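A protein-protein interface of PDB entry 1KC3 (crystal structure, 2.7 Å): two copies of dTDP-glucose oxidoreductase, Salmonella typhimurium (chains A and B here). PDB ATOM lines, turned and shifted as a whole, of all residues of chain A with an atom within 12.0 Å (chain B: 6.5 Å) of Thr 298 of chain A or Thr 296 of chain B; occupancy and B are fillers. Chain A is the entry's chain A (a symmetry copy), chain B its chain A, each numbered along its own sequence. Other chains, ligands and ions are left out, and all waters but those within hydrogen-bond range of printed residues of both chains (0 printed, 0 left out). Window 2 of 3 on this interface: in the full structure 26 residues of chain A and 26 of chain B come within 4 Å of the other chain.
The side-chain carboxylate (OE2) of Glu 292 of chain B is in hydrogen-bond range of the indole nitrogen (NE1) of Trp 14 of chain A, at 2.7 Å.
The backbone carbonyl oxygen (O) of Thr 291 of chain B lies within hydrogen-bond range of the side-chain hydroxyl (OG1) of Thr 295 of chain B, at 3.1 Å.
The backbone carbonyl oxygen (O) of Met 293 of chain B lies within hydrogen-bond range of the side-chain hydroxyl (OG1) of Thr 296 of chain B, 3.0 Å away.
O of Met 293 of chain A sits at hydrogen-bond distance from OG1 of Thr 296 of chain A (3.0 Å).
Among the printed residues, merely in contact across the chains: Trp 14 of chain A with Thr 291 of chain B (3.7 Å), Lys 158 of chain A with Thr 295 of chain B (3.6 Å), Thr 296 of chain A with Thr 298 of chain B (3.7 Å) and Thr 298 of chain A with Thr 296 of chain B (3.7 Å).
Thr 296 of chain B touches just one residue of chain A: Thr 298 (3.7 Å).
Met 293 of chain B touches none of the printed residues of chain A.
Thr 295 of chain B touches just one residue of chain A: Lys 158 (3.6 Å).
No residue of chain A comes within 4 Å of Thr 297 of chain B.
Of the printed residues of chain B, Thr 296 of chain A touches Thr 298 (3.7 Å).
Printed residues of chain B within 4 Å of Trp 14 of chain A: Thr 291 and Glu 292.
Phe 294 of chain B touches none of the printed residues of chain A.
Phe 294 of chain A touches none of the printed residues of chain B.
Printed residues of chain A that touch a printed residue of chain B: Trp 14, Lys 158, Thr 296 and Thr 298.
Among the printed residues, no Asp or Glu carboxylate lies within 4 Å of a Lys or Arg side-chain nitrogen of the other chain.
Thr 296 of chain A touches Thr 298 of chain B, and with the chains exchanged Thr 298 of chain A touches Thr 296 of chain B.
Positions printed for both chains: 168, 171, 291, 292, 293, 294, 295, 296, 297 and 298.
Of the 5 pairs that touch across the chains among the printed residues, 2 have their exchanged pair printed and touching as well.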
ATOM      1  N   TRP A  14      23.096  29.039  37.722  1.00  0.00           N
ATOM      2  CA  TRP A  14      21.976  28.630  36.839  1.00  0.00           C
ATOM      3  C   TRP A  14      20.739  28.457  37.686  1.00  0.00           C
ATOM      4  O   TRP A  14      19.687  28.750  37.278  1.00  0.00           O
ATOM      5  CB  TRP A  14      22.322  27.292  36.141  1.00  0.00           C
ATOM      6  CG  TRP A  14      21.288  26.690  35.226  1.00  0.00           C
ATOM      7  CD1 TRP A  14      20.559  25.577  35.436  1.00  0.00           C
ATOM      8  CD2 TRP A  14      20.926  27.191  33.956  1.00  0.00           C
ATOM      9  NE1 TRP A  14      19.735  25.354  34.361  1.00  0.00           N
ATOM     10  CE2 TRP A  14      19.911  26.372  33.465  1.00  0.00           C
ATOM     11  CE3 TRP A  14      21.294  28.329  33.226  1.00  0.00           C
ATOM     12  CZ2 TRP A  14      19.296  26.610  32.263  1.00  0.00           C
ATOM     13  CZ3 TRP A  14      20.688  28.578  32.060  1.00  0.00           C
ATOM     14  CH2 TRP A  14      19.713  27.692  31.552  1.00  0.00           C
ATOM     15  N   GLY A 157      22.513  19.278  38.549  1.00  0.00           N
ATOM     16  CA  GLY A 157      22.207  18.515  37.329  1.00  0.00           C
ATOM     17  C   GLY A 157      22.703  19.070  35.999  1.00  0.00           C
ATOM     18  O   GLY A 157      22.700  18.398  35.046  1.00  0.00           O
ATOM     19  N   LYS A 158      23.055  20.319  35.945  1.00  0.00           N
ATOM     20  CA  LYS A 158      23.606  20.992  34.779  1.00  0.00           C
ATOM     21  C   LYS A 158      24.930  21.659  35.295  1.00  0.00           C
ATOM     22  O   LYS A 158      24.968  22.691  35.972  1.00  0.00           O
ATOM     23  CB  LYS A 158      22.624  22.020  34.149  1.00  0.00           C
ATOM     24  CG  LYS A 158      23.307  23.077  33.235  1.00  0.00           C
ATOM     25  CD  LYS A 158      22.387  23.813  32.311  1.00  0.00           C
ATOM     26  CE  LYS A 158      23.114  24.852  31.409  1.00  0.00           C
ATOM     27  NZ  LYS A 158      23.763  24.348  30.157  1.00  0.00           N
ATOM     28  N   GLY A 159      26.032  21.067  34.948  1.00  0.00           N
ATOM     29  CA  GLY A 159      27.332  21.606  35.361  1.00  0.00           C
ATOM     30  C   GLY A 159      28.148  20.548  36.090  1.00  0.00           C
ATOM     31  O   GLY A 159      27.600  19.746  36.876  1.00  0.00           O
ATOM     32  N   ASN A 160      29.451  20.585  35.861  1.00  0.00           N
ATOM     33  CA  ASN A 160      30.364  19.539  36.375  1.00  0.00           C
ATOM     34  C   ASN A 160      30.529  19.460  37.917  1.00  0.00           C
ATOM     35  O   ASN A 160      30.761  20.464  38.610  1.00  0.00           O
ATOM     36  CB  ASN A 160      31.704  19.544  35.634  1.00  0.00           C
ATOM     37  CG  ASN A 160      31.509  19.396  34.131  1.00  0.00           C
ATOM     38  OD1 ASN A 160      32.019  20.199  33.353  1.00  0.00           O
ATOM     39  ND2 ASN A 160      30.693  18.417  33.726  1.00  0.00           N
ATOM     40  N   LYS A 164      28.630  13.581  38.725  1.00  0.00           N
ATOM     41  CA  LYS A 164      28.707  13.634  37.245  1.00  0.00           C
ATOM     42  C   LYS A 164      29.931  12.894  36.716  1.00  0.00           C
ATOM     43  O   LYS A 164      29.829  12.018  35.816  1.00  0.00           O
ATOM     44  CB  LYS A 164      28.773  15.079  36.673  1.00  0.00           C
ATOM     45  CG  LYS A 164      27.407  15.639  36.223  1.00  0.00           C
ATOM     46  CD  LYS A 164      27.456  16.579  35.002  1.00  0.00           C
ATOM     47  CE  LYS A 164      26.055  17.231  34.854  1.00  0.00           C
ATOM     48  NZ  LYS A 164      25.921  18.098  33.672  1.00  0.00           N
ATOM     49  N   ARG A 168      30.324   8.813  34.943  1.00  0.00           N
ATOM     50  CA  ARG A 168      30.960   8.684  33.604  1.00  0.00           C
ATOM     51  C   ARG A 168      31.981   7.514  33.603  1.00  0.00           C
ATOM     52  O   ARG A 168      32.026   6.680  32.675  1.00  0.00           O
ATOM     53  CB  ARG A 168      31.696   9.986  33.191  1.00  0.00           C
ATOM     54  CG  ARG A 168      30.934  10.953  32.270  1.00  0.00           C
ATOM     55  CD  ARG A 168      31.866  11.933  31.542  1.00  0.00           C
ATOM     56  NE  ARG A 168      32.895  11.260  30.691  1.00  0.00           N
ATOM     57  CZ  ARG A 168      32.710  10.720  29.456  1.00  0.00           C
ATOM     58  NH1 ARG A 168      31.529  10.733  28.844  1.00  0.00           N
ATOM     59  NH2 ARG A 168      33.732  10.168  28.832  1.00  0.00           N
ATOM     60  N   LYS A 171      30.307   3.852  34.196  1.00  0.00           N
ATOM     61  CA  LYS A 171      29.636   3.292  32.991  1.00  0.00           C
ATOM     62  C   LYS A 171      30.676   2.767  32.013  1.00  0.00           C
ATOM     63  O   LYS A 171      30.458   1.766  31.334  1.00  0.00           O
ATOM     64  CB  LYS A 171      28.683   4.297  32.293  1.00  0.00           C
ATOM     65  CG  LYS A 171      27.562   3.572  31.494  1.00  0.00           C
ATOM     66  CD  LYS A 171      26.624   4.547  30.817  1.00  0.00           C
ATOM     67  CE  LYS A 171      25.599   3.843  29.940  1.00  0.00           C
ATOM     68  NZ  LYS A 171      24.385   4.731  29.758  1.00  0.00           N
ATOM     69  N   THR A 291      17.560  11.458  39.412  1.00  0.00           N
ATOM     70  CA  THR A 291      16.308  11.025  38.752  1.00  0.00           C
ATOM     71  C   THR A 291      16.083  11.769  37.449  1.00  0.00           C
ATOM     72  O   THR A 291      15.700  11.192  36.445  1.00  0.00           O
ATOM     73  CB  THR A 291      15.156  11.269  39.629  1.00  0.00           C
ATOM     74  OG1 THR A 291      15.172  10.327  40.684  1.00  0.00           O
ATOM     75  CG2 THR A 291      13.855  11.012  38.964  1.00  0.00           C
ATOM     76  N   GLU A 292      16.309  13.067  37.508  1.00  0.00           N
ATOM     77  CA  GLU A 292      16.223  13.983  36.359  1.00  0.00           C
ATOM     78  C   GLU A 292      17.210  13.689  35.223  1.00  0.00           C
ATOM     79  O   GLU A 292      16.925  13.918  34.055  1.00  0.00           O
ATOM     80  CB  GLU A 292      16.434  15.419  36.837  1.00  0.00           C
ATOM     81  CG  GLU A 292      15.296  15.938  37.694  1.00  0.00           C
ATOM     82  CD  GLU A 292      15.374  17.424  37.955  1.00  0.00           C
ATOM     83  OE1 GLU A 292      16.493  17.973  38.133  1.00  0.00           O
ATOM     84  OE2 GLU A 292      14.302  18.032  38.026  1.00  0.00           O
ATOM     85  N   MET A 293      18.391  13.247  35.610  1.00  0.00           N
ATOM     86  CA  MET A 293      19.462  12.825  34.667  1.00  0.00           C
ATOM     87  C   MET A 293      19.071  11.515  33.977  1.00  0.00           C
ATOM     88  O   MET A 293      19.086  11.419  32.742  1.00  0.00           O
ATOM     89  CB  MET A 293      20.821  12.642  35.383  1.00  0.00           C
ATOM     90  CG  MET A 293      21.635  13.935  35.613  1.00  0.00           C
ATOM     91  SD  MET A 293      23.348  13.423  36.184  1.00  0.00           S
ATOM     92  CE  MET A 293      24.102  12.843  34.619  1.00  0.00           C
ATOM     93  N   PHE A 294      18.688  10.532  34.799  1.00  0.00           N
ATOM     94  CA  PHE A 294      18.150   9.219  34.322  1.00  0.00           C
ATOM     95  C   PHE A 294      16.763   9.260  33.667  1.00  0.00           C
ATOM     96  O   PHE A 294      16.214   8.211  33.362  1.00  0.00           O
ATOM     97  CB  PHE A 294      18.090   8.138  35.416  1.00  0.00           C
ATOM     98  CG  PHE A 294      19.335   8.002  36.215  1.00  0.00           C
ATOM     99  CD1 PHE A 294      20.598   8.214  35.653  1.00  0.00           C
ATOM    100  CD2 PHE A 294      19.235   7.679  37.554  1.00  0.00           C
ATOM    101  CE1 PHE A 294      21.715   8.108  36.402  1.00  0.00           C
ATOM    102  CE2 PHE A 294      20.360   7.550  38.316  1.00  0.00           C
ATOM    103  CZ  PHE A 294      21.614   7.762  37.739  1.00  0.00           C
ATOM    104  N   THR A 295      16.156  10.429  33.536  1.00  0.00           N
ATOM    105  CA  THR A 295      15.012  10.572  32.646  1.00  0.00           C
ATOM    106  C   THR A 295      15.666  11.019  31.315  1.00  0.00           C
ATOM    107  O   THR A 295      15.795  12.223  31.042  1.00  0.00           O
ATOM    108  CB  THR A 295      13.960  11.503  33.158  1.00  0.00           C
ATOM    109  OG1 THR A 295      13.409  10.925  34.353  1.00  0.00           O
ATOM    110  CG2 THR A 295      12.769  11.567  32.184  1.00  0.00           C
ATOM    111  N   THR A 296      16.074   9.999  30.533  1.00  0.00           N
ATOM    112  CA  THR A 296      16.804  10.126  29.245  1.00  0.00           C
ATOM    113  C   THR A 296      15.947   9.873  27.989  1.00  0.00           C
ATOM    114  O   THR A 296      16.076   8.834  27.274  1.00  0.00           O
ATOM    115  CB  THR A 296      18.109   9.235  29.225  1.00  0.00           C
ATOM    116  OG1 THR A 296      19.007   9.680  30.264  1.00  0.00           O
ATOM    117  CG2 THR A 296      18.951   9.426  27.928  1.00  0.00           C
ATOM    118  N   THR A 297      15.059  10.833  27.755  1.00  0.00           N
ATOM    119  CA  THR A 297      14.374  10.972  26.445  1.00  0.00           C
ATOM    120  C   THR A 297      13.984  12.459  26.180  1.00  0.00           C
ATOM    121  O   THR A 297      13.504  13.193  27.078  1.00  0.00           O
ATOM    122  CB  THR A 297      13.201   9.914  26.136  1.00  0.00           C
ATOM    123  OG1 THR A 297      13.750   8.650  25.686  1.00  0.00           O
ATOM    124  CG2 THR A 297      12.347  10.324  24.908  1.00  0.00           C
ATOM    125  N   THR A 298      14.253  12.819  24.910  1.00  0.00           N
ATOM    126  CA  THR A 298      13.942  14.100  24.212  1.00  0.00           C
ATOM    127  C   THR A 298      12.686  13.949  23.303  1.00  0.00           C
ATOM    128  O   THR A 298      12.722  13.329  22.226  1.00  0.00           O
ATOM    129  CB  THR A 298      15.153  14.589  23.303  1.00  0.00           C
ATOM    130  OG1 THR A 298      16.423  14.390  23.960  1.00  0.00           O
ATOM    131  CG2 THR A 298      15.087  16.109  23.028  1.00  0.00           C
ATOM    132  N   ARG B 168       8.038  17.474  19.557  1.00  0.00           N
ATOM    133  CA  ARG B 168       8.050  16.061  19.091  1.00  0.00           C
ATOM    134  C   ARG B 168       7.555  15.976  17.621  1.00  0.00           C
ATOM    135  O   ARG B 168       8.150  15.287  16.766  1.00  0.00           O
ATOM    136  CB  ARG B 168       7.145  15.160  19.972  1.00  0.00           C
ATOM    137  CG  ARG B 168       7.839  14.356  21.084  1.00  0.00           C
ATOM    138  CD  ARG B 168       6.994  13.169  21.570  1.00  0.00           C
ATOM    139  NE  ARG B 168       6.658  12.192  20.489  1.00  0.00           N
ATOM    140  CZ  ARG B 168       7.471  11.234  19.969  1.00  0.00           C
ATOM    141  NH1 ARG B 168       8.722  11.057  20.390  1.00  0.00           N
ATOM    142  NH2 ARG B 168       7.014  10.442  19.019  1.00  0.00           N
ATOM    143  N   LYS B 171       9.976  17.860  14.947  1.00  0.00           N
ATOM    144  CA  LYS B 171      11.204  17.094  14.598  1.00  0.00           C
ATOM    145  C   LYS B 171      10.858  15.965  13.639  1.00  0.00           C
ATOM    146  O   LYS B 171      11.638  15.629  12.751  1.00  0.00           O
ATOM    147  CB  LYS B 171      11.963  16.551  15.836  1.00  0.00           C
ATOM    148  CG  LYS B 171      13.477  16.341  15.542  1.00  0.00           C
ATOM    149  CD  LYS B 171      14.224  15.818  16.748  1.00  0.00           C
ATOM    150  CE  LYS B 171      15.678  15.502  16.429  1.00  0.00           C
ATOM    151  NZ  LYS B 171      16.502  15.543  17.700  1.00  0.00           N
ATOM    152  N   ILE B 239      19.572  22.100  16.299  1.00  0.00           N
ATOM    153  CA  ILE B 239      18.800  20.881  16.016  1.00  0.00           C
ATOM    154  C   ILE B 239      18.219  20.893  14.614  1.00  0.00           C
ATOM    155  O   ILE B 239      17.534  21.864  14.257  1.00  0.00           O
ATOM    156  CB  ILE B 239      17.644  20.681  17.029  1.00  0.00           C
ATOM    157  CG1 ILE B 239      18.206  20.219  18.371  1.00  0.00           C
ATOM    158  CG2 ILE B 239      16.601  19.664  16.483  1.00  0.00           C
ATOM    159  CD1 ILE B 239      17.164  20.006  19.441  1.00  0.00           C
ATOM    160  N   THR B 291      16.439  25.221  27.259  1.00  0.00           N
ATOM    161  CA  THR B 291      17.915  25.120  27.294  1.00  0.00           C
ATOM    162  C   THR B 291      18.367  23.836  27.964  1.00  0.00           C
ATOM    163  O   THR B 291      19.274  23.164  27.505  1.00  0.00           O
ATOM    164  CB  THR B 291      18.488  26.253  28.030  1.00  0.00           C
ATOM    165  OG1 THR B 291      18.378  27.420  27.239  1.00  0.00           O
ATOM    166  CG2 THR B 291      19.951  26.126  28.244  1.00  0.00           C
ATOM    167  N   GLU B 292      17.722  23.537  29.075  1.00  0.00           N
ATOM    168  CA  GLU B 292      17.937  22.312  29.862  1.00  0.00           C
ATOM    169  C   GLU B 292      17.622  21.006  29.123  1.00  0.00           C
ATOM    170  O   GLU B 292      18.243  19.977  29.355  1.00  0.00           O
ATOM    171  CB  GLU B 292      17.098  22.373  31.137  1.00  0.00           C
ATOM    172  CG  GLU B 292      17.576  23.424  32.120  1.00  0.00           C
ATOM    173  CD  GLU B 292      16.919  23.319  33.475  1.00  0.00           C
ATOM    174  OE1 GLU B 292      15.705  22.996  33.562  1.00  0.00           O
ATOM    175  OE2 GLU B 292      17.615  23.606  34.453  1.00  0.00           O
ATOM    176  N   MET B 293      16.601  21.067  28.291  1.00  0.00           N
ATOM    177  CA  MET B 293      16.180  19.938  27.418  1.00  0.00           C
ATOM    178  C   MET B 293      17.216  19.715  26.312  1.00  0.00           C
ATOM    179  O   MET B 293      17.712  18.594  26.123  1.00  0.00           O
ATOM    180  CB  MET B 293      14.794  20.188  26.780  1.00  0.00           C
ATOM    181  CG  MET B 293      13.578  19.852  27.671  1.00  0.00           C
ATOM    182  SD  MET B 293      12.050  19.923  26.584  1.00  0.00           S
ATOM    183  CE  MET B 293      12.196  18.361  25.639  1.00  0.00           C
ATOM    184  N   PHE B 294      17.553  20.807  25.618  1.00  0.00           N
ATOM    185  CA  PHE B 294      18.633  20.829  24.583  1.00  0.00           C
ATOM    186  C   PHE B 294      20.067  20.675  25.106  1.00  0.00           C
ATOM    187  O   PHE B 294      21.004  20.801  24.330  1.00  0.00           O
ATOM    188  CB  PHE B 294      18.619  22.087  23.696  1.00  0.00           C
ATOM    189  CG  PHE B 294      17.283  22.440  23.151  1.00  0.00           C
ATOM    190  CD1 PHE B 294      16.342  21.461  22.815  1.00  0.00           C
ATOM    191  CD2 PHE B 294      16.958  23.774  22.996  1.00  0.00           C
ATOM    192  CE1 PHE B 294      15.125  21.805  22.345  1.00  0.00           C
ATOM    193  CE2 PHE B 294      15.737  24.131  22.501  1.00  0.00           C
ATOM    194  CZ  PHE B 294      14.810  23.142  22.168  1.00  0.00           C
ATOM    195  N   THR B 295      20.256  20.503  26.404  1.00  0.00           N
ATOM    196  CA  THR B 295      21.538  20.031  26.909  1.00  0.00           C
ATOM    197  C   THR B 295      21.341  18.496  26.965  1.00  0.00           C
ATOM    198  O   THR B 295      20.938  17.943  28.002  1.00  0.00           O
ATOM    199  CB  THR B 295      21.940  20.648  28.210  1.00  0.00           C
ATOM    200  OG1 THR B 295      22.144  22.053  27.983  1.00  0.00           O
ATOM    201  CG2 THR B 295      23.321  20.131  28.654  1.00  0.00           C
ATOM    202  N   THR B 296      21.627  17.862  25.810  1.00  0.00           N
ATOM    203  CA  THR B 296      21.454  16.410  25.547  1.00  0.00           C
ATOM    204  C   THR B 296      22.761  15.592  25.548  1.00  0.00           C
ATOM    205  O   THR B 296      23.268  15.115  24.488  1.00  0.00           O
ATOM    206  CB  THR B 296      20.631  16.153  24.222  1.00  0.00           C
ATOM    207  OG1 THR B 296      19.309  16.716  24.364  1.00  0.00           O
ATOM    208  CG2 THR B 296      20.343  14.642  23.973  1.00  0.00           C
ATOM    209  N   THR B 297      23.299  15.463  26.755  1.00  0.00           N
ATOM    210  CA  THR B 297      24.349  14.455  27.047  1.00  0.00           C
ATOM    211  C   THR B 297      24.297  14.020  28.545  1.00  0.00           C
ATOM    212  O   THR B 297      24.123  14.845  29.474  1.00  0.00           O
ATOM    213  CB  THR B 297      25.828  14.784  26.504  1.00  0.00           C
ATOM    214  OG1 THR B 297      25.945  14.462  25.095  1.00  0.00           O
ATOM    215  CG2 THR B 297      26.902  13.849  27.116  1.00  0.00           C
ATOM    216  N   THR B 298      24.438  12.686  28.674  1.00  0.00           N
ATOM    217  CA  THR B 298      24.553  11.871  29.918  1.00  0.00           C
ATOM    218  C   THR B 298      26.036  11.482  30.195  1.00  0.00           C
ATOM    219  O   THR B 298      26.625  10.614  29.528  1.00  0.00           O
ATOM    220  CB  THR B 298      23.699  10.532  29.831  1.00  0.00           C
ATOM    221  OG1 THR B 298      22.416  10.760  29.209  1.00  0.00           O
ATOM    222  CG2 THR B 298      23.360   9.974  31.233  1.00  0.00           C
